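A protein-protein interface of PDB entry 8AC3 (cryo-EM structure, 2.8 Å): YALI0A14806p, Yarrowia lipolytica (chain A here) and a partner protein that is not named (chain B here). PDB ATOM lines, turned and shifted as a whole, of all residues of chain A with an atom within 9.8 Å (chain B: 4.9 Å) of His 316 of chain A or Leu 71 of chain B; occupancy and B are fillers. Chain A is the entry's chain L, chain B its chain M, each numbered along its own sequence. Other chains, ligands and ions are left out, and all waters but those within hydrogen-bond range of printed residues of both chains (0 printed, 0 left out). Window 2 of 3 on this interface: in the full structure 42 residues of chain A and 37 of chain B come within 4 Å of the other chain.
O of His 316 of chain A lies within hydrogen-bond range of NE of Arg 75 of chain B, at 2.7 Å.
N of Gly 318 of chain A is in hydrogen-bond range of OE2 of Glu 78 of chain B, at 3.2 Å.
O of Asn 306 of chain A sits at hydrogen-bond distance from NE2 of Gln 317 of chain A (2.8 Å).
NE2 of Gln 317 of chain A is in hydrogen-bond range of OG of Ser 322 of chain A (3.1 Å).
ND2 of Asn 323 of chain A lies within hydrogen-bond range of O of Gln 317 of chain A, 3.1 Å away.
O of Gly 318 of chain A is in hydrogen-bond range of ND2 of Asn 323 of chain A (3.5 Å).
The side-chain amide oxygen (OD1) of Asn 64 of chain B is in hydrogen-bond range of the backbone NH (N) of Ala 70 of chain B, 2.8 Å away.
O of Thr 313 of chain A touches CG1 of Val 74 of chain B, at 3.8 Å.
Arg 128 of chain B touches Arg 315 of chain A.
His 316 of chain A touches Ala 70 of chain B (NE2 to CB, 3.9 Å).
His 316 of chain A touches Leu 71 of chain B.
O of His 316 of chain A touches CG1 of Val 74 of chain B, at 3.7 Å.
NH1 of Arg 128 of chain B touches CE1 of His 316 of chain A (3.8 Å).
C of Gln 317 of chain A touches NE of Arg 75 of chain B, 3.6 Å away.
Glu 78 of chain B touches Gln 317 of chain A (OE1 to CB, 3.6 Å).
Gly 318 of chain A touches Arg 75 of chain B.
O of Glu 78 of chain B touches CB of Gln 388 of chain A, at 3.7 Å.
His 316 of chain A touches just these residues of chain B: Ala 70, Leu 71, Val 74, Arg 75 and Arg 128.
Of the printed residues of chain A, Leu 71 of chain B touches His 316.
No residue of chain A comes within 4 Å of Ser 69 of chain B.
Ala 70 of chain B touches just one residue of chain A: His 316 (3.9 Å).
Printed residues of chain B within 4 Å of Gln 388 of chain A: Glu 78.
Printed residues of chain A within 4 Å of Arg 75 of chain B: His 316 (2.7 Å), Gln 317 (3.6 Å) and Gly 318 (3.5 Å).
Of the printed residues of chain B, Thr 313 of chain A touches Val 74 (3.8 Å).
Of the printed residues of chain B, Gly 318 of chain A touches Arg 75 (3.5 Å) and Glu 78 (3.2 Å).
Of the printed residues of chain B, Gln 317 of chain A touches Arg 75 (3.6 Å) and Glu 78 (3.6 Å).
The nearest residue of chain B that does not touch His 316 of chain A is Glu 78 of chain B (4.2 Å).
Printed residues of chain A that touch a printed residue of chain B: Thr 313, Arg 315, His 316, Gln 317, Gly 318 and Gln 388.
Hydrophobic or aromatic side chains of chain A that line the printed part of chain B: His 316.
Along chain A the printed residues that touch a printed residue of chain B span positions 313 to 388.
Printed residues of chain B that touch a printed residue of chain A: Ala 70, Leu 71, Val 74, Arg 75, Glu 78 and Arg 128.
Among the printed residues, 12 pairs touch across the chains.
Among the printed residues, no Asp or Glu carboxylate lies within 4 Å of a Lys or Arg side-chain nitrogen of the other chain.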
ATOM      1  N   ASN A 306     -12.381  17.111 -20.828  1.00  0.00           N
ATOM      2  CA  ASN A 306     -13.082  16.845 -19.588  1.00  0.00           C
ATOM      3  C   ASN A 306     -12.275  15.850 -18.778  1.00  0.00           C
ATOM      4  O   ASN A 306     -11.383  15.202 -19.308  1.00  0.00           O
ATOM      5  CB  ASN A 306     -14.457  16.260 -19.862  1.00  0.00           C
ATOM      6  CG  ASN A 306     -15.279  17.213 -20.695  1.00  0.00           C
ATOM      7  OD1 ASN A 306     -15.195  18.426 -20.514  1.00  0.00           O
ATOM      8  ND2 ASN A 306     -16.069  16.679 -21.609  1.00  0.00           N
ATOM      9  N   TYR A 307     -12.563  15.775 -17.488  1.00  0.00           N
ATOM     10  CA  TYR A 307     -11.885  14.824 -16.641  1.00  0.00           C
ATOM     11  C   TYR A 307     -12.808  14.492 -15.485  1.00  0.00           C
ATOM     12  O   TYR A 307     -13.440  15.398 -14.959  1.00  0.00           O
ATOM     13  CB  TYR A 307     -10.650  15.482 -16.041  1.00  0.00           C
ATOM     14  CG  TYR A 307     -10.045  14.651 -14.947  1.00  0.00           C
ATOM     15  CD1 TYR A 307      -9.304  13.516 -15.251  1.00  0.00           C
ATOM     16  CD2 TYR A 307     -10.260  14.957 -13.613  1.00  0.00           C
ATOM     17  CE1 TYR A 307      -8.736  12.739 -14.254  1.00  0.00           C
ATOM     18  CE2 TYR A 307      -9.704  14.185 -12.604  1.00  0.00           C
ATOM     19  CZ  TYR A 307      -8.949  13.069 -12.926  1.00  0.00           C
ATOM     20  OH  TYR A 307      -8.403  12.297 -11.942  1.00  0.00           O
ATOM     21  N   ASP A 308     -12.844  13.224 -15.063  1.00  0.00           N
ATOM     22  CA  ASP A 308     -13.625  12.866 -13.891  1.00  0.00           C
ATOM     23  C   ASP A 308     -12.928  11.732 -13.160  1.00  0.00           C
ATOM     24  O   ASP A 308     -12.765  10.668 -13.733  1.00  0.00           O
ATOM     25  CB  ASP A 308     -15.036  12.445 -14.296  1.00  0.00           C
ATOM     26  CG  ASP A 308     -15.950  12.054 -13.147  1.00  0.00           C
ATOM     27  OD1 ASP A 308     -15.663  12.432 -11.981  1.00  0.00           O
ATOM     28  OD2 ASP A 308     -16.970  11.383 -13.429  1.00  0.00           O
ATOM     29  N   ARG A 309     -12.567  11.929 -11.889  1.00  0.00           N
ATOM     30  CA  ARG A 309     -11.810  10.904 -11.183  1.00  0.00           C
ATOM     31  C   ARG A 309     -12.606   9.604 -11.038  1.00  0.00           C
ATOM     32  O   ARG A 309     -12.029   8.533 -10.884  1.00  0.00           O
ATOM     33  CB  ARG A 309     -11.187  11.437  -9.890  1.00  0.00           C
ATOM     34  CG  ARG A 309     -12.174  11.555  -8.744  1.00  0.00           C
ATOM     35  CD  ARG A 309     -11.532  11.722  -7.393  1.00  0.00           C
ATOM     36  NE  ARG A 309     -12.756  11.892  -6.629  1.00  0.00           N
ATOM     37  CZ  ARG A 309     -12.850  12.166  -5.334  1.00  0.00           C
ATOM     38  NH1 ARG A 309     -11.768  12.322  -4.588  1.00  0.00           N
ATOM     39  NH2 ARG A 309     -14.049  12.289  -4.791  1.00  0.00           N
ATOM     40  N   VAL A 311     -14.381   8.204 -13.348  1.00  0.00           N
ATOM     41  CA  VAL A 311     -14.421   7.411 -14.563  1.00  0.00           C
ATOM     42  C   VAL A 311     -13.083   6.698 -14.688  1.00  0.00           C
ATOM     43  O   VAL A 311     -12.050   7.302 -14.433  1.00  0.00           O
ATOM     44  CB  VAL A 311     -14.748   8.308 -15.766  1.00  0.00           C
ATOM     45  CG1 VAL A 311     -14.524   7.618 -17.100  1.00  0.00           C
ATOM     46  CG2 VAL A 311     -16.178   8.807 -15.667  1.00  0.00           C
ATOM     47  N   GLY A 312     -13.105   5.418 -15.071  1.00  0.00           N
ATOM     48  CA  GLY A 312     -11.893   4.606 -15.082  1.00  0.00           C
ATOM     49  C   GLY A 312     -10.825   5.101 -16.061  1.00  0.00           C
ATOM     50  O   GLY A 312      -9.634   5.163 -15.737  1.00  0.00           O
ATOM     51  N   THR A 313     -11.275   5.467 -17.260  1.00  0.00           N
ATOM     52  CA  THR A 313     -10.389   5.800 -18.362  1.00  0.00           C
ATOM     53  C   THR A 313      -9.751   7.176 -18.188  1.00  0.00           C
ATOM     54  O   THR A 313      -8.791   7.481 -18.884  1.00  0.00           O
ATOM     55  CB  THR A 313     -11.143   5.744 -19.693  1.00  0.00           C
ATOM     56  OG1 THR A 313     -12.150   6.756 -19.658  1.00  0.00           O
ATOM     57  CG2 THR A 313     -11.759   4.388 -19.947  1.00  0.00           C
ATOM     58  N   SER A 314     -10.272   8.003 -17.276  1.00  0.00           N
ATOM     59  CA  SER A 314      -9.905   9.411 -17.267  1.00  0.00           C
ATOM     60  C   SER A 314      -8.434   9.621 -16.912  1.00  0.00           C
ATOM     61  O   SER A 314      -7.830  10.600 -17.322  1.00  0.00           O
ATOM     62  CB  SER A 314     -10.807  10.214 -16.384  1.00  0.00           C
ATOM     63  OG  SER A 314     -10.580   9.859 -15.033  1.00  0.00           O
ATOM     64  N   ARG A 315      -7.831   8.697 -16.168  1.00  0.00           N
ATOM     65  CA  ARG A 315      -6.431   8.897 -15.842  1.00  0.00           C
ATOM     66  C   ARG A 315      -5.529   8.689 -17.060  1.00  0.00           C
ATOM     67  O   ARG A 315      -4.342   8.999 -17.017  1.00  0.00           O
ATOM     68  CB  ARG A 315      -6.034   7.978 -14.700  1.00  0.00           C
ATOM     69  CG  ARG A 315      -5.823   6.538 -15.133  1.00  0.00           C
ATOM     70  CD  ARG A 315      -5.084   5.838 -14.020  1.00  0.00           C
ATOM     71  NE  ARG A 315      -5.982   5.636 -12.888  1.00  0.00           N
ATOM     72  CZ  ARG A 315      -5.804   6.111 -11.658  1.00  0.00           C
ATOM     73  NH1 ARG A 315      -4.715   6.797 -11.341  1.00  0.00           N
ATOM     74  NH2 ARG A 315      -6.711   5.863 -10.731  1.00  0.00           N
ATOM     75  N   HIS A 316      -6.086   8.190 -18.163  1.00  0.00           N
ATOM     76  CA  HIS A 316      -5.246   7.887 -19.305  1.00  0.00           C
ATOM     77  C   HIS A 316      -5.508   8.827 -20.465  1.00  0.00           C
ATOM     78  O   HIS A 316      -4.966   8.603 -21.544  1.00  0.00           O
ATOM     79  CB  HIS A 316      -5.507   6.464 -19.767  1.00  0.00           C
ATOM     80  CG  HIS A 316      -5.090   5.478 -18.748  1.00  0.00           C
ATOM     81  ND1 HIS A 316      -3.820   5.497 -18.203  1.00  0.00           N
ATOM     82  CD2 HIS A 316      -5.766   4.472 -18.153  1.00  0.00           C
ATOM     83  CE1 HIS A 316      -3.723   4.530 -17.323  1.00  0.00           C
ATOM     84  NE2 HIS A 316      -4.902   3.882 -17.273  1.00  0.00           N
ATOM     85  N   GLN A 317      -6.336   9.846 -20.255  1.00  0.00           N
ATOM     86  CA  GLN A 317      -6.656  10.775 -21.329  1.00  0.00           C
ATOM     87  C   GLN A 317      -5.414  11.535 -21.791  1.00  0.00           C
ATOM     88  O   GLN A 317      -4.467  11.750 -21.035  1.00  0.00           O
ATOM     89  CB  GLN A 317      -7.718  11.757 -20.864  1.00  0.00           C
ATOM     90  CG  GLN A 317      -9.049  11.081 -20.625  1.00  0.00           C
ATOM     91  CD  GLN A 317     -10.098  12.072 -20.183  1.00  0.00           C
ATOM     92  OE1 GLN A 317     -11.210  12.090 -20.709  1.00  0.00           O
ATOM     93  NE2 GLN A 317      -9.765  12.899 -19.200  1.00  0.00           N
ATOM     94  N   GLY A 318      -5.449  11.976 -23.050  1.00  0.00           N
ATOM     95  CA  GLY A 318      -4.287  12.583 -23.671  1.00  0.00           C
ATOM     96  C   GLY A 318      -4.066  14.044 -23.289  1.00  0.00           C
ATOM     97  O   GLY A 318      -2.929  14.518 -23.351  1.00  0.00           O
ATOM     98  N   SER A 319      -5.164  14.756 -22.997  1.00  0.00           N
ATOM     99  CA  SER A 319      -5.195  16.147 -22.559  1.00  0.00           C
ATOM    100  C   SER A 319      -4.125  16.434 -21.507  1.00  0.00           C
ATOM    101  O   SER A 319      -4.033  15.728 -20.505  1.00  0.00           O
ATOM    102  CB  SER A 319      -6.568  16.477 -22.020  1.00  0.00           C
ATOM    103  OG  SER A 319      -6.556  17.687 -21.268  1.00  0.00           O
ATOM    104  N   ARG A 320      -3.346  17.504 -21.718  1.00  0.00           N
ATOM    105  CA  ARG A 320      -2.269  17.853 -20.806  1.00  0.00           C
ATOM    106  C   ARG A 320      -2.827  18.225 -19.431  1.00  0.00           C
ATOM    107  O   ARG A 320      -2.284  17.824 -18.399  1.00  0.00           O
ATOM    108  CB  ARG A 320      -1.372  18.930 -21.426  1.00  0.00           C
ATOM    109  CG  ARG A 320      -0.326  19.491 -20.477  1.00  0.00           C
ATOM    110  CD  ARG A 320       0.693  18.445 -20.066  1.00  0.00           C
ATOM    111  NE  ARG A 320       1.651  18.991 -19.112  1.00  0.00           N
ATOM    112  CZ  ARG A 320       2.556  18.288 -18.429  1.00  0.00           C
ATOM    113  NH1 ARG A 320       2.646  16.976 -18.581  1.00  0.00           N
ATOM    114  NH2 ARG A 320       3.371  18.906 -17.590  1.00  0.00           N
ATOM    115  N   SER A 322      -5.559  17.180 -18.121  1.00  0.00           N
ATOM    116  CA  SER A 322      -6.035  15.953 -17.512  1.00  0.00           C
ATOM    117  C   SER A 322      -4.881  15.257 -16.797  1.00  0.00           C
ATOM    118  O   SER A 322      -5.032  14.827 -15.653  1.00  0.00           O
ATOM    119  CB  SER A 322      -6.657  15.063 -18.532  1.00  0.00           C
ATOM    120  OG  SER A 322      -7.159  13.893 -17.911  1.00  0.00           O
ATOM    121  N   ASN A 323      -3.722  15.213 -17.459  1.00  0.00           N
ATOM    122  CA  ASN A 323      -2.573  14.565 -16.860  1.00  0.00           C
ATOM    123  C   ASN A 323      -2.133  15.285 -15.595  1.00  0.00           C
ATOM    124  O   ASN A 323      -1.890  14.636 -14.589  1.00  0.00           O
ATOM    125  CB  ASN A 323      -1.443  14.340 -17.856  1.00  0.00           C
ATOM    126  CG  ASN A 323      -1.844  13.274 -18.846  1.00  0.00           C
ATOM    127  OD1 ASN A 323      -1.886  12.096 -18.498  1.00  0.00           O
ATOM    128  ND2 ASN A 323      -2.177  13.671 -20.065  1.00  0.00           N
ATOM    129  N   ILE A 324      -2.029  16.612 -15.647  1.00  0.00           N
ATOM    130  CA  ILE A 324      -1.544  17.354 -14.494  1.00  0.00           C
ATOM    131  C   ILE A 324      -2.488  17.132 -13.316  1.00  0.00           C
ATOM    132  O   ILE A 324      -2.060  16.993 -12.176  1.00  0.00           O
ATOM    133  CB  ILE A 324      -1.439  18.853 -14.836  1.00  0.00           C
ATOM    134  CG1 ILE A 324      -0.319  19.151 -15.837  1.00  0.00           C
ATOM    135  CG2 ILE A 324      -1.294  19.681 -13.567  1.00  0.00           C
ATOM    136  CD1 ILE A 324      -0.567  20.388 -16.672  1.00  0.00           C
ATOM    137  N   SER A 326      -4.765  14.761 -12.762  1.00  0.00           N
ATOM    138  CA  SER A 326      -4.860  13.415 -12.229  1.00  0.00           C
ATOM    139  C   SER A 326      -3.617  13.042 -11.424  1.00  0.00           C
ATOM    140  O   SER A 326      -3.767  12.484 -10.344  1.00  0.00           O
ATOM    141  CB  SER A 326      -5.206  12.406 -13.281  1.00  0.00           C
ATOM    142  OG  SER A 326      -4.170  12.312 -14.242  1.00  0.00           O
ATOM    143  N   GLU A 327      -2.414  13.392 -11.912  1.00  0.00           N
ATOM    144  CA  GLU A 327      -1.163  13.038 -11.238  1.00  0.00           C
ATOM    145  C   GLU A 327      -1.060  13.716  -9.873  1.00  0.00           C
ATOM    146  O   GLU A 327      -0.520  13.153  -8.922  1.00  0.00           O
ATOM    147  CB  GLU A 327       0.066  13.402 -12.074  1.00  0.00           C
ATOM    148  CG  GLU A 327       0.209  12.565 -13.332  1.00  0.00           C
ATOM    149  CD  GLU A 327       1.308  13.007 -14.288  1.00  0.00           C
ATOM    150  OE1 GLU A 327       1.243  14.150 -14.799  1.00  0.00           O
ATOM    151  OE2 GLU A 327       2.238  12.205 -14.516  1.00  0.00           O
ATOM    152  N   ARG A 384      -5.646  15.587 -33.161  1.00  0.00           N
ATOM    153  CA  ARG A 384      -6.199  14.672 -32.180  1.00  0.00           C
ATOM    154  C   ARG A 384      -7.619  15.097 -31.788  1.00  0.00           C
ATOM    155  O   ARG A 384      -8.490  14.246 -31.616  1.00  0.00           O
ATOM    156  CB  ARG A 384      -5.289  14.611 -30.953  1.00  0.00           C
ATOM    157  CG  ARG A 384      -3.961  13.881 -31.129  1.00  0.00           C
ATOM    158  CD  ARG A 384      -3.267  13.513 -29.822  1.00  0.00           C
ATOM    159  NE  ARG A 384      -2.824  14.658 -29.034  1.00  0.00           N
ATOM    160  CZ  ARG A 384      -3.212  14.997 -27.801  1.00  0.00           C
ATOM    161  NH1 ARG A 384      -2.729  16.100 -27.251  1.00  0.00           N
ATOM    162  NH2 ARG A 384      -4.057  14.249 -27.107  1.00  0.00           N
ATOM    163  N   GLN A 388     -11.552  13.360 -32.337  1.00  0.00           N
ATOM    164  CA  GLN A 388     -12.444  13.125 -31.226  1.00  0.00           C
ATOM    165  C   GLN A 388     -13.788  13.818 -31.440  1.00  0.00           C
ATOM    166  O   GLN A 388     -14.771  13.380 -30.851  1.00  0.00           O
ATOM    167  CB  GLN A 388     -11.734  13.634 -29.979  1.00  0.00           C
ATOM    168  CG  GLN A 388     -12.539  13.513 -28.702  1.00  0.00           C
ATOM    169  CD  GLN A 388     -11.578  13.442 -27.547  1.00  0.00           C
ATOM    170  OE1 GLN A 388     -10.458  13.945 -27.617  1.00  0.00           O
ATOM    171  NE2 GLN A 388     -12.002  12.778 -26.488  1.00  0.00           N
ATOM    172  N   ASN B  64      -4.892  -3.377 -18.363  1.00  0.00           N
ATOM    173  CA  ASN B  64      -3.774  -3.819 -19.176  1.00  0.00           C
ATOM    174  C   ASN B  64      -4.034  -5.224 -19.695  1.00  0.00           C
ATOM    175  O   ASN B  64      -4.348  -6.135 -18.945  1.00  0.00           O
ATOM    176  CB  ASN B  64      -2.457  -3.801 -18.412  1.00  0.00           C
ATOM    177  CG  ASN B  64      -2.047  -2.411 -17.982  1.00  0.00           C
ATOM    178  OD1 ASN B  64      -2.299  -1.432 -18.683  1.00  0.00           O
ATOM    179  ND2 ASN B  64      -1.391  -2.312 -16.837  1.00  0.00           N
ATOM    180  N   SER B  69      -1.821  -1.958 -23.612  1.00  0.00           N
ATOM    181  CA  SER B  69      -1.954  -1.430 -22.265  1.00  0.00           C
ATOM    182  C   SER B  69      -3.238  -0.620 -22.158  1.00  0.00           C
ATOM    183  O   SER B  69      -3.758  -0.139 -23.159  1.00  0.00           O
ATOM    184  CB  SER B  69      -0.780  -0.576 -21.908  1.00  0.00           C
ATOM    185  OG  SER B  69      -0.804   0.620 -22.664  1.00  0.00           O
ATOM    186  N   ALA B  70      -3.716  -0.448 -20.925  1.00  0.00           N
ATOM    187  CA  ALA B  70      -4.876   0.392 -20.687  1.00  0.00           C
ATOM    188  C   ALA B  70      -4.647   1.777 -21.283  1.00  0.00           C
ATOM    189  O   ALA B  70      -5.529   2.316 -21.949  1.00  0.00           O
ATOM    190  CB  ALA B  70      -5.179   0.462 -19.214  1.00  0.00           C
ATOM    191  N   LEU B  71      -3.446   2.319 -21.055  1.00  0.00           N
ATOM    192  CA  LEU B  71      -3.077   3.616 -21.584  1.00  0.00           C
ATOM    193  C   LEU B  71      -3.176   3.631 -23.104  1.00  0.00           C
ATOM    194  O   LEU B  71      -3.814   4.521 -23.663  1.00  0.00           O
ATOM    195  CB  LEU B  71      -1.657   3.947 -21.131  1.00  0.00           C
ATOM    196  CG  LEU B  71      -1.047   5.171 -21.799  1.00  0.00           C
ATOM    197  CD1 LEU B  71      -1.865   6.414 -21.489  1.00  0.00           C
ATOM    198  CD2 LEU B  71       0.376   5.348 -21.316  1.00  0.00           C
ATOM    199  N   ARG B  72      -2.550   2.661 -23.774  1.00  0.00           N
ATOM    200  CA  ARG B  72      -2.599   2.704 -25.222  1.00  0.00           C
ATOM    201  C   ARG B  72      -4.035   2.590 -25.730  1.00  0.00           C
ATOM    202  O   ARG B  72      -4.408   3.223 -26.714  1.00  0.00           O
ATOM    203  CB  ARG B  72      -1.778   1.594 -25.864  1.00  0.00           C
ATOM    204  CG  ARG B  72      -1.745   1.785 -27.369  1.00  0.00           C
ATOM    205  CD  ARG B  72      -0.526   1.337 -28.144  1.00  0.00           C
ATOM    206  NE  ARG B  72       0.766   1.809 -27.651  1.00  0.00           N
ATOM    207  CZ  ARG B  72       1.645   2.544 -28.336  1.00  0.00           C
ATOM    208  NH1 ARG B  72       1.386   2.929 -29.576  1.00  0.00           N
ATOM    209  NH2 ARG B  72       2.788   2.889 -27.770  1.00  0.00           N
ATOM    210  N   PHE B  73      -4.840   1.761 -25.075  1.00  0.00           N
ATOM    211  CA  PHE B  73      -6.210   1.604 -25.520  1.00  0.00           C
ATOM    212  C   PHE B  73      -6.958   2.931 -25.427  1.00  0.00           C
ATOM    213  O   PHE B  73      -7.602   3.337 -26.392  1.00  0.00           O
ATOM    214  CB  PHE B  73      -6.929   0.526 -24.714  1.00  0.00           C
ATOM    215  CG  PHE B  73      -8.386   0.415 -25.079  1.00  0.00           C
ATOM    216  CD1 PHE B  73      -8.767  -0.113 -26.307  1.00  0.00           C
ATOM    217  CD2 PHE B  73      -9.371   0.885 -24.219  1.00  0.00           C
ATOM    218  CE1 PHE B  73     -10.109  -0.177 -26.658  1.00  0.00           C
ATOM    219  CE2 PHE B  73     -10.715   0.799 -24.560  1.00  0.00           C
ATOM    220  CZ  PHE B  73     -11.081   0.275 -25.783  1.00  0.00           C
ATOM    221  N   VAL B  74      -6.883   3.590 -24.270  1.00  0.00           N
ATOM    222  CA  VAL B  74      -7.598   4.838 -24.086  1.00  0.00           C
ATOM    223  C   VAL B  74      -7.148   5.885 -25.105  1.00  0.00           C
ATOM    224  O   VAL B  74      -7.989   6.589 -25.653  1.00  0.00           O
ATOM    225  CB  VAL B  74      -7.477   5.351 -22.644  1.00  0.00           C
ATOM    226  CG1 VAL B  74      -7.984   6.784 -22.498  1.00  0.00           C
ATOM    227  CG2 VAL B  74      -8.190   4.430 -21.674  1.00  0.00           C
ATOM    228  N   ARG B  75      -5.842   6.017 -25.352  1.00  0.00           N
ATOM    229  CA  ARG B  75      -5.400   7.053 -26.275  1.00  0.00           C
ATOM    230  C   ARG B  75      -5.843   6.730 -27.702  1.00  0.00           C
ATOM    231  O   ARG B  75      -6.028   7.635 -28.513  1.00  0.00           O
ATOM    232  CB  ARG B  75      -3.878   7.215 -26.291  1.00  0.00           C
ATOM    233  CG  ARG B  75      -3.250   7.677 -24.989  1.00  0.00           C
ATOM    234  CD  ARG B  75      -3.703   9.058 -24.589  1.00  0.00           C
ATOM    235  NE  ARG B  75      -3.055   9.358 -23.334  1.00  0.00           N
ATOM    236  CZ  ARG B  75      -1.918  10.030 -23.223  1.00  0.00           C
ATOM    237  NH1 ARG B  75      -1.304  10.481 -24.303  1.00  0.00           N
ATOM    238  NH2 ARG B  75      -1.394  10.245 -22.029  1.00  0.00           N
ATOM    239  N   GLU B  78      -9.597   7.478 -28.190  1.00  0.00           N
ATOM    240  CA  GLU B  78      -9.795   8.917 -28.341  1.00  0.00           C
ATOM    241  C   GLU B  78      -9.538   9.357 -29.781  1.00  0.00           C
ATOM    242  O   GLU B  78     -10.145  10.315 -30.238  1.00  0.00           O
ATOM    243  CB  GLU B  78      -8.878   9.727 -27.421  1.00  0.00           C
ATOM    244  CG  GLU B  78      -9.256   9.705 -25.943  1.00  0.00           C
ATOM    245  CD  GLU B  78      -8.265  10.378 -24.985  1.00  0.00           C
ATOM    246  OE1 GLU B  78      -8.660  11.328 -24.260  1.00  0.00           O
ATOM    247  OE2 GLU B  78      -7.097   9.914 -24.938  1.00  0.00           O
ATOM    248  N   ARG B 128      -6.240   1.259  -9.105  1.00  0.00           N
ATOM    249  CA  ARG B 128      -7.106   1.696 -10.183  1.00  0.00           C
ATOM    250  C   ARG B 128      -8.524   1.172  -9.993  1.00  0.00           C
ATOM    251  O   ARG B 128      -9.454   1.960  -9.873  1.00  0.00           O
ATOM    252  CB  ARG B 128      -6.464   1.335 -11.520  1.00  0.00           C
ATOM    253  CG  ARG B 128      -5.122   2.025 -11.672  1.00  0.00           C
ATOM    254  CD  ARG B 128      -4.411   1.473 -12.872  1.00  0.00           C
ATOM    255  NE  ARG B 128      -3.268   2.344 -13.068  1.00  0.00           N
ATOM    256  CZ  ARG B 128      -2.516   2.386 -14.158  1.00  0.00           C
ATOM    257  NH1 ARG B 128      -2.767   1.593 -15.188  1.00  0.00           N
ATOM    258  NH2 ARG B 128      -1.506   3.236 -14.212  1.00  0.00           N
